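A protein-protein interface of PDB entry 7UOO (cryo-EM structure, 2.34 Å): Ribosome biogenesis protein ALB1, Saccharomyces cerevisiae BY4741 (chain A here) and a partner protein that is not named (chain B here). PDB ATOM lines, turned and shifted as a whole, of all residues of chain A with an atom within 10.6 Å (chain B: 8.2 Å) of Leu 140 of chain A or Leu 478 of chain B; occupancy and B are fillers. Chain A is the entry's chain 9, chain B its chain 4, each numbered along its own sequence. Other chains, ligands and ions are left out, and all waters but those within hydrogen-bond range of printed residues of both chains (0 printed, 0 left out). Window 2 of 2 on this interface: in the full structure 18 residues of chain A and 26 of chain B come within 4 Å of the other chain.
The side-chain amino group of Lys 144 of chain A lies within hydrogen-bond range of the backbone carbonyl oxygen of Leu 449 of chain B, 2.4 Å away.
The backbone NH of Leu 478 of chain B is in hydrogen-bond range of the side-chain carboxylate of Glu 275 of chain B (3.0 Å). The side-chain hydroxyl (OG) of Ser 138 of chain A sits close to the backbone NH (N) of Leu 140 of chain A, at 3.4 Å.
Leu 140 of chain A touches Leu 478 of chain B. Leu 279 of chain B touches Val 143 of chain A. Val 143 of chain A touches Leu 478 of chain B. Leu 279 of chain B touches Leu 147 of chain A. CD2 of Leu 147 of chain A touches CD2 of Leu 449 of chain B (3.7 Å). Leu 147 of chain A touches Leu 478 of chain B. CG1 of Val 150 of chain A touches O of Leu 278 of chain B, at 3.6 Å. Ile 151 of chain A touches Leu 278 of chain B. Trp 445 of chain B touches Ile 151 of chain A (CB to CD1, 3.97 Å). Ile 151 of chain A touches Leu 449 of chain B (CD1 to CD1, 3.8 Å).
Of the printed residues of chain B, Val 143 of chain A touches Leu 279 and Leu 478. Printed residues of chain B within 4 Å of Val 150 of chain A: Leu 278. Of the printed residues of chain A, Trp 445 of chain B touches Leu 147 (3.9 Å) and Ile 151 (3.97 Å). No residue of chain A comes within 4 Å of Leu 475 of chain B. No residue of chain A comes within 4 Å of Pro 476 of chain B. Of chain A, only Leu 140, Val 143, Lys 144 and Leu 147 come within 4 Å of Leu 478 of chain B. No residue of chain A comes within 4 Å of Gly 479 of chain B. No residue of chain A comes within 4 Å of Val 480 of chain B. The nearest residue of chain B that does not touch Leu 140 of chain A is Lys 477 of chain B (4.5 Å). The nearest printed residue of chain B that does not touch Val 143 of chain A is Lys 477 of chain B (4.5 Å).
Of the 23 printed residues of chain B, 5 touch a printed residue of chain A. Of the 13 printed residues of chain A, 8 touch a printed residue of chain B. Hydrophobic or aromatic side chains of chain A that line the printed part of chain B: Leu 140, Val 143, Ala 146, Leu 147, Trp 148, Val 150 and Ile 151.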
ATOM      1  N   SER A 138      -6.061  -6.927  35.101  1.00  0.00           N
ATOM      2  CA  SER A 138      -6.189  -6.398  33.747  1.00  0.00           C
ATOM      3  C   SER A 138      -5.053  -5.433  33.435  1.00  0.00           C
ATOM      4  O   SER A 138      -4.648  -4.646  34.287  1.00  0.00           O
ATOM      5  CB  SER A 138      -7.539  -5.698  33.569  1.00  0.00           C
ATOM      6  OG  SER A 138      -7.651  -5.119  32.280  1.00  0.00           O
ATOM      7  N   SER A 139      -4.534  -5.508  32.206  1.00  0.00           N
ATOM      8  CA  SER A 139      -3.466  -4.599  31.802  1.00  0.00           C
ATOM      9  C   SER A 139      -3.954  -3.157  31.759  1.00  0.00           C
ATOM     10  O   SER A 139      -3.228  -2.239  32.162  1.00  0.00           O
ATOM     11  CB  SER A 139      -2.905  -5.019  30.444  1.00  0.00           C
ATOM     12  OG  SER A 139      -1.787  -4.222  30.091  1.00  0.00           O
ATOM     13  N   LEU A 140      -5.177  -2.938  31.269  1.00  0.00           N
ATOM     14  CA  LEU A 140      -5.745  -1.594  31.267  1.00  0.00           C
ATOM     15  C   LEU A 140      -5.915  -1.070  32.685  1.00  0.00           C
ATOM     16  O   LEU A 140      -5.632   0.103  32.962  1.00  0.00           O
ATOM     17  CB  LEU A 140      -7.085  -1.592  30.530  1.00  0.00           C
ATOM     18  CG  LEU A 140      -7.819  -0.252  30.429  1.00  0.00           C
ATOM     19  CD1 LEU A 140      -6.995   0.754  29.650  1.00  0.00           C
ATOM     20  CD2 LEU A 140      -9.187  -0.438  29.787  1.00  0.00           C
ATOM     21  N   THR A 141      -6.366  -1.932  33.601  1.00  0.00           N
ATOM     22  CA  THR A 141      -6.495  -1.536  34.998  1.00  0.00           C
ATOM     23  C   THR A 141      -5.140  -1.187  35.600  1.00  0.00           C
ATOM     24  O   THR A 141      -5.013  -0.189  36.316  1.00  0.00           O
ATOM     25  CB  THR A 141      -7.168  -2.652  35.800  1.00  0.00           C
ATOM     26  OG1 THR A 141      -8.432  -2.975  35.210  1.00  0.00           O
ATOM     27  CG2 THR A 141      -7.388  -2.216  37.238  1.00  0.00           C
ATOM     28  N   LEU A 142      -4.111  -1.991  35.309  1.00  0.00           N
ATOM     29  CA  LEU A 142      -2.777  -1.705  35.831  1.00  0.00           C
ATOM     30  C   LEU A 142      -2.241  -0.382  35.295  1.00  0.00           C
ATOM     31  O   LEU A 142      -1.656   0.410  36.048  1.00  0.00           O
ATOM     32  CB  LEU A 142      -1.820  -2.847  35.487  1.00  0.00           C
ATOM     33  CG  LEU A 142      -2.013  -4.187  36.202  1.00  0.00           C
ATOM     34  CD1 LEU A 142      -1.005  -5.203  35.698  1.00  0.00           C
ATOM     35  CD2 LEU A 142      -1.905  -4.025  37.711  1.00  0.00           C
ATOM     36  N   VAL A 143      -2.441  -0.121  34.001  1.00  0.00           N
ATOM     37  CA  VAL A 143      -1.974   1.129  33.405  1.00  0.00           C
ATOM     38  C   VAL A 143      -2.701   2.323  34.014  1.00  0.00           C
ATOM     39  O   VAL A 143      -2.084   3.346  34.334  1.00  0.00           O
ATOM     40  CB  VAL A 143      -2.135   1.084  31.873  1.00  0.00           C
ATOM     41  CG1 VAL A 143      -1.895   2.457  31.263  1.00  0.00           C
ATOM     42  CG2 VAL A 143      -1.173   0.072  31.275  1.00  0.00           C
ATOM     43  N   LYS A 144      -4.021   2.212  34.192  1.00  0.00           N
ATOM     44  CA  LYS A 144      -4.778   3.316  34.776  1.00  0.00           C
ATOM     45  C   LYS A 144      -4.386   3.556  36.231  1.00  0.00           C
ATOM     46  O   LYS A 144      -4.289   4.709  36.670  1.00  0.00           O
ATOM     47  CB  LYS A 144      -6.278   3.051  34.648  1.00  0.00           C
ATOM     48  CG  LYS A 144      -6.788   3.122  33.213  1.00  0.00           C
ATOM     49  CD  LYS A 144      -8.250   2.723  33.115  1.00  0.00           C
ATOM     50  CE  LYS A 144      -9.166   3.820  33.629  1.00  0.00           C
ATOM     51  NZ  LYS A 144      -9.208   4.983  32.701  1.00  0.00           N
ATOM     52  N   GLU A 145      -4.145   2.483  36.990  1.00  0.00           N
ATOM     53  CA  GLU A 145      -3.688   2.635  38.368  1.00  0.00           C
ATOM     54  C   GLU A 145      -2.323   3.307  38.431  1.00  0.00           C
ATOM     55  O   GLU A 145      -2.095   4.185  39.272  1.00  0.00           O
ATOM     56  CB  GLU A 145      -3.642   1.274  39.065  1.00  0.00           C
ATOM     57  CG  GLU A 145      -5.006   0.666  39.338  1.00  0.00           C
ATOM     58  CD  GLU A 145      -5.891   1.569  40.167  1.00  0.00           C
ATOM     59  OE1 GLU A 145      -5.390   2.153  41.151  1.00  0.00           O
ATOM     60  OE2 GLU A 145      -7.087   1.702  39.832  1.00  0.00           O
ATOM     61  N   ALA A 146      -1.402   2.909  37.549  1.00  0.00           N
ATOM     62  CA  ALA A 146      -0.085   3.540  37.523  1.00  0.00           C
ATOM     63  C   ALA A 146      -0.185   5.013  37.142  1.00  0.00           C
ATOM     64  O   ALA A 146       0.498   5.860  37.730  1.00  0.00           O
ATOM     65  CB  ALA A 146       0.836   2.793  36.560  1.00  0.00           C
ATOM     66  N   LEU A 147      -1.037   5.340  36.166  1.00  0.00           N
ATOM     67  CA  LEU A 147      -1.206   6.736  35.772  1.00  0.00           C
ATOM     68  C   LEU A 147      -1.796   7.566  36.903  1.00  0.00           C
ATOM     69  O   LEU A 147      -1.367   8.703  37.136  1.00  0.00           O
ATOM     70  CB  LEU A 147      -2.083   6.835  34.524  1.00  0.00           C
ATOM     71  CG  LEU A 147      -1.356   7.170  33.218  1.00  0.00           C
ATOM     72  CD1 LEU A 147      -0.576   5.969  32.711  1.00  0.00           C
ATOM     73  CD2 LEU A 147      -2.328   7.670  32.160  1.00  0.00           C
ATOM     74  N   TRP A 148      -2.782   7.022  37.620  1.00  0.00           N
ATOM     75  CA  TRP A 148      -3.358   7.759  38.741  1.00  0.00           C
ATOM     76  C   TRP A 148      -2.343   7.936  39.863  1.00  0.00           C
ATOM     77  O   TRP A 148      -2.278   9.003  40.487  1.00  0.00           O
ATOM     78  CB  TRP A 148      -4.615   7.060  39.254  1.00  0.00           C
ATOM     79  CG  TRP A 148      -5.383   7.893  40.235  1.00  0.00           C
ATOM     80  CD1 TRP A 148      -5.348   7.800  41.596  1.00  0.00           C
ATOM     81  CD2 TRP A 148      -6.290   8.961  39.929  1.00  0.00           C
ATOM     82  NE1 TRP A 148      -6.182   8.738  42.156  1.00  0.00           N
ATOM     83  CE2 TRP A 148      -6.772   9.462  41.155  1.00  0.00           C
ATOM     84  CE3 TRP A 148      -6.744   9.537  38.738  1.00  0.00           C
ATOM     85  CZ2 TRP A 148      -7.686  10.514  41.224  1.00  0.00           C
ATOM     86  CZ3 TRP A 148      -7.649  10.579  38.808  1.00  0.00           C
ATOM     87  CH2 TRP A 148      -8.111  11.058  40.043  1.00  0.00           C
ATOM     88  N   VAL A 150       0.836   8.183  39.458  1.00  0.00           N
ATOM     89  CA  VAL A 150       1.893   9.092  39.030  1.00  0.00           C
ATOM     90  C   VAL A 150       1.399  10.522  38.814  1.00  0.00           C
ATOM     91  O   VAL A 150       2.219  11.451  38.798  1.00  0.00           O
ATOM     92  CB  VAL A 150       2.584   8.554  37.760  1.00  0.00           C
ATOM     93  CG1 VAL A 150       1.812   8.930  36.508  1.00  0.00           C
ATOM     94  CG2 VAL A 150       4.026   9.041  37.681  1.00  0.00           C
ATOM     95  N   ILE A 151       0.091  10.733  38.658  1.00  0.00           N
ATOM     96  CA  ILE A 151      -0.432  12.094  38.575  1.00  0.00           C
ATOM     97  C   ILE A 151      -0.962  12.606  39.911  1.00  0.00           C
ATOM     98  O   ILE A 151      -1.079  13.829  40.086  1.00  0.00           O
ATOM     99  CB  ILE A 151      -1.529  12.227  37.496  1.00  0.00           C
ATOM    100  CG1 ILE A 151      -2.795  11.472  37.908  1.00  0.00           C
ATOM    101  CG2 ILE A 151      -1.009  11.767  36.142  1.00  0.00           C
ATOM    102  CD1 ILE A 151      -3.918  11.564  36.903  1.00  0.00           C
ATOM    103  N   GLU B 271       1.554  12.648  21.350  1.00  0.00           N
ATOM    104  CA  GLU B 271       0.805  12.347  22.567  1.00  0.00           C
ATOM    105  C   GLU B 271       1.154  10.966  23.106  1.00  0.00           C
ATOM    106  O   GLU B 271       1.129  10.752  24.322  1.00  0.00           O
ATOM    107  CB  GLU B 271      -0.699  12.442  22.308  1.00  0.00           C
ATOM    108  CG  GLU B 271      -1.172  13.769  21.737  1.00  0.00           C
ATOM    109  CD  GLU B 271      -1.247  13.760  20.224  1.00  0.00           C
ATOM    110  OE1 GLU B 271      -0.852  12.745  19.612  1.00  0.00           O
ATOM    111  OE2 GLU B 271      -1.705  14.764  19.643  1.00  0.00           O
ATOM    112  N   GLU B 275       2.435  10.152  26.837  1.00  0.00           N
ATOM    113  CA  GLU B 275       1.919   9.055  27.651  1.00  0.00           C
ATOM    114  C   GLU B 275       3.046   8.153  28.138  1.00  0.00           C
ATOM    115  O   GLU B 275       3.062   7.736  29.303  1.00  0.00           O
ATOM    116  CB  GLU B 275       0.898   8.256  26.838  1.00  0.00           C
ATOM    117  CG  GLU B 275       0.274   7.067  27.545  1.00  0.00           C
ATOM    118  CD  GLU B 275      -0.561   6.215  26.602  1.00  0.00           C
ATOM    119  OE1 GLU B 275      -0.234   6.167  25.400  1.00  0.00           O
ATOM    120  OE2 GLU B 275      -1.546   5.600  27.059  1.00  0.00           O
ATOM    121  N   LEU B 278       4.978   9.969  30.897  1.00  0.00           N
ATOM    122  CA  LEU B 278       4.239   9.960  32.155  1.00  0.00           C
ATOM    123  C   LEU B 278       4.247   8.580  32.802  1.00  0.00           C
ATOM    124  O   LEU B 278       4.336   8.474  34.030  1.00  0.00           O
ATOM    125  CB  LEU B 278       2.805  10.430  31.927  1.00  0.00           C
ATOM    126  CG  LEU B 278       2.004  10.708  33.197  1.00  0.00           C
ATOM    127  CD1 LEU B 278       2.638  11.844  33.982  1.00  0.00           C
ATOM    128  CD2 LEU B 278       0.557  11.023  32.865  1.00  0.00           C
ATOM    129  N   LEU B 279       4.161   7.517  32.000  1.00  0.00           N
ATOM    130  CA  LEU B 279       4.136   6.160  32.528  1.00  0.00           C
ATOM    131  C   LEU B 279       5.526   5.614  32.842  1.00  0.00           C
ATOM    132  O   LEU B 279       5.632   4.583  33.515  1.00  0.00           O
ATOM    133  CB  LEU B 279       3.420   5.241  31.533  1.00  0.00           C
ATOM    134  CG  LEU B 279       2.891   3.887  32.008  1.00  0.00           C
ATOM    135  CD1 LEU B 279       2.411   3.968  33.443  1.00  0.00           C
ATOM    136  CD2 LEU B 279       1.766   3.434  31.103  1.00  0.00           C
ATOM    137  N   LEU B 334      -2.351  16.700  29.107  1.00  0.00           N
ATOM    138  CA  LEU B 334      -1.861  16.239  27.817  1.00  0.00           C
ATOM    139  C   LEU B 334      -1.998  17.348  26.781  1.00  0.00           C
ATOM    140  O   LEU B 334      -3.021  18.036  26.728  1.00  0.00           O
ATOM    141  CB  LEU B 334      -2.632  14.996  27.363  1.00  0.00           C
ATOM    142  CG  LEU B 334      -2.309  14.386  25.998  1.00  0.00           C
ATOM    143  CD1 LEU B 334      -0.920  13.787  25.990  1.00  0.00           C
ATOM    144  CD2 LEU B 334      -3.343  13.339  25.622  1.00  0.00           C
ATOM    145  N   TRP B 445      -5.200  14.831  32.615  1.00  0.00           N
ATOM    146  CA  TRP B 445      -5.157  13.373  32.614  1.00  0.00           C
ATOM    147  C   TRP B 445      -6.290  12.748  33.417  1.00  0.00           C
ATOM    148  O   TRP B 445      -6.686  11.612  33.130  1.00  0.00           O
ATOM    149  CB  TRP B 445      -3.814  12.880  33.155  1.00  0.00           C
ATOM    150  CG  TRP B 445      -2.687  13.029  32.185  1.00  0.00           C
ATOM    151  CD1 TRP B 445      -1.697  13.963  32.219  1.00  0.00           C
ATOM    152  CD2 TRP B 445      -2.438  12.223  31.028  1.00  0.00           C
ATOM    153  NE1 TRP B 445      -0.844  13.789  31.158  1.00  0.00           N
ATOM    154  CE2 TRP B 445      -1.278  12.726  30.410  1.00  0.00           C
ATOM    155  CE3 TRP B 445      -3.084  11.122  30.456  1.00  0.00           C
ATOM    156  CZ2 TRP B 445      -0.749  12.169  29.251  1.00  0.00           C
ATOM    157  CZ3 TRP B 445      -2.557  10.572  29.304  1.00  0.00           C
ATOM    158  CH2 TRP B 445      -1.402  11.095  28.713  1.00  0.00           C
ATOM    159  N   ILE B 448      -9.298  12.136  31.206  1.00  0.00           N
ATOM    160  CA  ILE B 448      -9.034  11.024  30.295  1.00  0.00           C
ATOM    161  C   ILE B 448      -9.152   9.692  31.024  1.00  0.00           C
ATOM    162  O   ILE B 448      -9.727   8.730  30.502  1.00  0.00           O
ATOM    163  CB  ILE B 448      -7.649  11.194  29.641  1.00  0.00           C
ATOM    164  CG1 ILE B 448      -7.595  12.494  28.839  1.00  0.00           C
ATOM    165  CG2 ILE B 448      -7.314  10.002  28.749  1.00  0.00           C
ATOM    166  CD1 ILE B 448      -6.276  12.724  28.134  1.00  0.00           C
ATOM    167  N   LEU B 449      -8.610   9.615  32.242  1.00  0.00           N
ATOM    168  CA  LEU B 449      -8.672   8.368  32.998  1.00  0.00           C
ATOM    169  C   LEU B 449     -10.098   8.048  33.436  1.00  0.00           C
ATOM    170  O   LEU B 449     -10.514   6.884  33.400  1.00  0.00           O
ATOM    171  CB  LEU B 449      -7.737   8.439  34.204  1.00  0.00           C
ATOM    172  CG  LEU B 449      -6.243   8.425  33.876  1.00  0.00           C
ATOM    173  CD1 LEU B 449      -5.410   8.606  35.132  1.00  0.00           C
ATOM    174  CD2 LEU B 449      -5.865   7.140  33.161  1.00  0.00           C
ATOM    175  N   ALA B 451     -12.782   8.910  31.874  1.00  0.00           N
ATOM    176  CA  ALA B 451     -13.621   8.662  30.713  1.00  0.00           C
ATOM    177  C   ALA B 451     -13.667   7.175  30.366  1.00  0.00           C
ATOM    178  O   ALA B 451     -12.776   6.395  30.712  1.00  0.00           O
ATOM    179  CB  ALA B 451     -13.114   9.452  29.514  1.00  0.00           C
ATOM    180  N   ASN B 453     -14.408   4.471  27.032  1.00  0.00           N
ATOM    181  CA  ASN B 453     -14.566   4.262  25.592  1.00  0.00           C
ATOM    182  C   ASN B 453     -15.002   2.826  25.337  1.00  0.00           C
ATOM    183  O   ASN B 453     -14.202   1.894  25.539  1.00  0.00           O
ATOM    184  CB  ASN B 453     -13.275   4.583  24.836  1.00  0.00           C
ATOM    185  CG  ASN B 453     -12.045   4.004  25.497  1.00  0.00           C
ATOM    186  OD1 ASN B 453     -12.020   3.788  26.708  1.00  0.00           O
ATOM    187  ND2 ASN B 453     -11.013   3.753  24.704  1.00  0.00           N
ATOM    188  N   GLY B 456     -12.529   1.188  22.420  1.00  0.00           N
ATOM    189  CA  GLY B 456     -11.107   1.044  22.663  1.00  0.00           C
ATOM    190  C   GLY B 456     -10.242   1.275  21.439  1.00  0.00           C
ATOM    191  O   GLY B 456     -10.301   2.343  20.823  1.00  0.00           O
ATOM    192  N   ASN B 457      -9.433   0.276  21.081  1.00  0.00           N
ATOM    193  CA  ASN B 457      -8.543   0.398  19.930  1.00  0.00           C
ATOM    194  C   ASN B 457      -9.301   0.406  18.608  1.00  0.00           C
ATOM    195  O   ASN B 457      -8.794   0.935  17.613  1.00  0.00           O
ATOM    196  CB  ASN B 457      -7.533  -0.749  19.920  1.00  0.00           C
ATOM    197  CG  ASN B 457      -6.402  -0.538  20.893  1.00  0.00           C
ATOM    198  OD1 ASN B 457      -6.067   0.596  21.235  1.00  0.00           O
ATOM    199  ND2 ASN B 457      -5.796  -1.629  21.340  1.00  0.00           N
ATOM    200  N   LEU B 473      -3.796   6.404  16.703  1.00  0.00           N
ATOM    201  CA  LEU B 473      -3.867   6.006  18.108  1.00  0.00           C
ATOM    202  C   LEU B 473      -2.987   6.952  18.914  1.00  0.00           C
ATOM    203  O   LEU B 473      -1.802   6.667  19.142  1.00  0.00           O
ATOM    204  CB  LEU B 473      -3.434   4.556  18.306  1.00  0.00           C
ATOM    205  CG  LEU B 473      -4.503   3.478  18.116  1.00  0.00           C
ATOM    206  CD1 LEU B 473      -3.974   2.118  18.539  1.00  0.00           C
ATOM    207  CD2 LEU B 473      -5.767   3.826  18.885  1.00  0.00           C
ATOM    208  N   PRO B 474      -3.519   8.095  19.350  1.00  0.00           N
ATOM    209  CA  PRO B 474      -2.705   9.017  20.155  1.00  0.00           C
ATOM    210  C   PRO B 474      -2.303   8.455  21.508  1.00  0.00           C
ATOM    211  O   PRO B 474      -1.289   8.888  22.067  1.00  0.00           O
ATOM    212  CB  PRO B 474      -3.611  10.248  20.296  1.00  0.00           C
ATOM    213  CG  PRO B 474      -4.993   9.721  20.123  1.00  0.00           C
ATOM    214  CD  PRO B 474      -4.880   8.608  19.122  1.00  0.00           C
ATOM    215  N   LEU B 475      -3.063   7.508  22.056  1.00  0.00           N
ATOM    216  CA  LEU B 475      -2.753   6.876  23.340  1.00  0.00           C
ATOM    217  C   LEU B 475      -2.840   5.364  23.177  1.00  0.00           C
ATOM    218  O   LEU B 475      -3.866   4.752  23.504  1.00  0.00           O
ATOM    219  CB  LEU B 475      -3.691   7.371  24.441  1.00  0.00           C
ATOM    220  CG  LEU B 475      -3.636   8.868  24.747  1.00  0.00           C
ATOM    221  CD1 LEU B 475      -4.689   9.250  25.772  1.00  0.00           C
ATOM    222  CD2 LEU B 475      -2.251   9.264  25.226  1.00  0.00           C
ATOM    223  N   PRO B 476      -1.785   4.732  22.651  1.00  0.00           N
ATOM    224  CA  PRO B 476      -1.836   3.274  22.431  1.00  0.00           C
ATOM    225  C   PRO B 476      -1.982   2.457  23.703  1.00  0.00           C
ATOM    226  O   PRO B 476      -2.675   1.431  23.696  1.00  0.00           O
ATOM    227  CB  PRO B 476      -0.501   2.981  21.729  1.00  0.00           C
ATOM    228  CG  PRO B 476      -0.023   4.296  21.219  1.00  0.00           C
ATOM    229  CD  PRO B 476      -0.512   5.311  22.197  1.00  0.00           C
ATOM    230  N   LYS B 477      -1.350   2.879  24.799  1.00  0.00           N
ATOM    231  CA  LYS B 477      -1.387   2.077  26.019  1.00  0.00           C
ATOM    232  C   LYS B 477      -2.753   2.140  26.687  1.00  0.00           C
ATOM    233  O   LYS B 477      -3.244   1.129  27.203  1.00  0.00           O
ATOM    234  CB  LYS B 477      -0.288   2.529  26.979  1.00  0.00           C
ATOM    235  CG  LYS B 477       1.098   2.039  26.590  1.00  0.00           C
ATOM    236  CD  LYS B 477       2.146   2.479  27.595  1.00  0.00           C
ATOM    237  CE  LYS B 477       3.493   1.826  27.321  1.00  0.00           C
ATOM    238  NZ  LYS B 477       4.057   2.212  26.002  1.00  0.00           N
ATOM    239  N   LEU B 478      -3.386   3.313  26.689  1.00  0.00           N
ATOM    240  CA  LEU B 478      -4.744   3.432  27.201  1.00  0.00           C
ATOM    241  C   LEU B 478      -5.794   3.002  26.185  1.00  0.00           C
ATOM    242  O   LEU B 478      -6.963   2.855  26.555  1.00  0.00           O
ATOM    243  CB  LEU B 478      -5.019   4.871  27.642  1.00  0.00           C
ATOM    244  CG  LEU B 478      -4.280   5.362  28.888  1.00  0.00           C
ATOM    245  CD1 LEU B 478      -4.341   6.877  28.984  1.00  0.00           C
ATOM    246  CD2 LEU B 478      -4.862   4.723  30.137  1.00  0.00           C
ATOM    247  N   GLY B 479      -5.409   2.791  24.932  1.00  0.00           N
ATOM    248  CA  GLY B 479      -6.360   2.433  23.896  1.00  0.00           C
ATOM    249  C   GLY B 479      -7.353   3.524  23.560  1.00  0.00           C
ATOM    250  O   GLY B 479      -8.545   3.240  23.391  1.00  0.00           O
ATOM    251  N   VAL B 480      -6.894   4.768  23.462  1.00  0.00           N
ATOM    252  CA  VAL B 480      -7.750   5.911  23.165  1.00  0.00           C
ATOM    253  C   VAL B 480      -7.425   6.393  21.760  1.00  0.00           C
ATOM    254  O   VAL B 480      -6.275   6.742  21.465  1.00  0.00           O
ATOM    255  CB  VAL B 480      -7.569   7.040  24.191  1.00  0.00           C
ATOM    256  CG1 VAL B 480      -8.515   8.191  23.883  1.00  0.00           C
ATOM    257  CG2 VAL B 480      -7.795   6.519  25.601  1.00  0.00           C
ATOM    258  N   SER B 481      -8.435   6.420  20.899  1.00  0.00           N
ATOM    259  CA  SER B 481      -8.271   6.838  19.517  1.00  0.00           C
ATOM    260  C   SER B 481      -8.381   8.357  19.392  1.00  0.00           C
ATOM    261  O   SER B 481      -8.681   9.068  20.352  1.00  0.00           O
ATOM    262  CB  SER B 481      -9.306   6.150  18.629  1.00  0.00           C
ATOM    263  OG  SER B 481     -10.623   6.454  19.054  1.00  0.00           O
ATOM    264  N   LYS B 484     -12.015   9.561  19.889  1.00  0.00           N
ATOM    265  CA  LYS B 484     -12.317   9.572  21.316  1.00  0.00           C
ATOM    266  C   LYS B 484     -11.613  10.727  22.019  1.00  0.00           C
ATOM    267  O   LYS B 484     -12.186  11.353  22.916  1.00  0.00           O
ATOM    268  CB  LYS B 484     -11.926   8.238  21.950  1.00  0.00           C
ATOM    269  CG  LYS B 484     -12.371   8.095  23.395  1.00  0.00           C
ATOM    270  CD  LYS B 484     -13.867   8.326  23.531  1.00  0.00           C
ATOM    271  CE  LYS B 484     -14.306   8.284  24.981  1.00  0.00           C
ATOM    272  NZ  LYS B 484     -15.750   8.613  25.134  1.00  0.00           N
ATOM    273  N   LEU B 488     -13.198  13.746  24.168  1.00  0.00           N
ATOM    274  CA  LEU B 488     -12.773  14.108  25.519  1.00  0.00           C
ATOM    275  C   LEU B 488     -12.438  15.591  25.619  1.00  0.00           C
ATOM    276  O   LEU B 488     -12.805  16.254  26.598  1.00  0.00           O
ATOM    277  CB  LEU B 488     -11.565  13.273  25.939  1.00  0.00           C
ATOM    278  CG  LEU B 488     -11.740  11.757  26.015  1.00  0.00           C
ATOM    279  CD1 LEU B 488     -10.628  11.113  26.828  1.00  0.00           C
ATOM    280  CD2 LEU B 488     -13.106  11.414  26.570  1.00  0.00           C
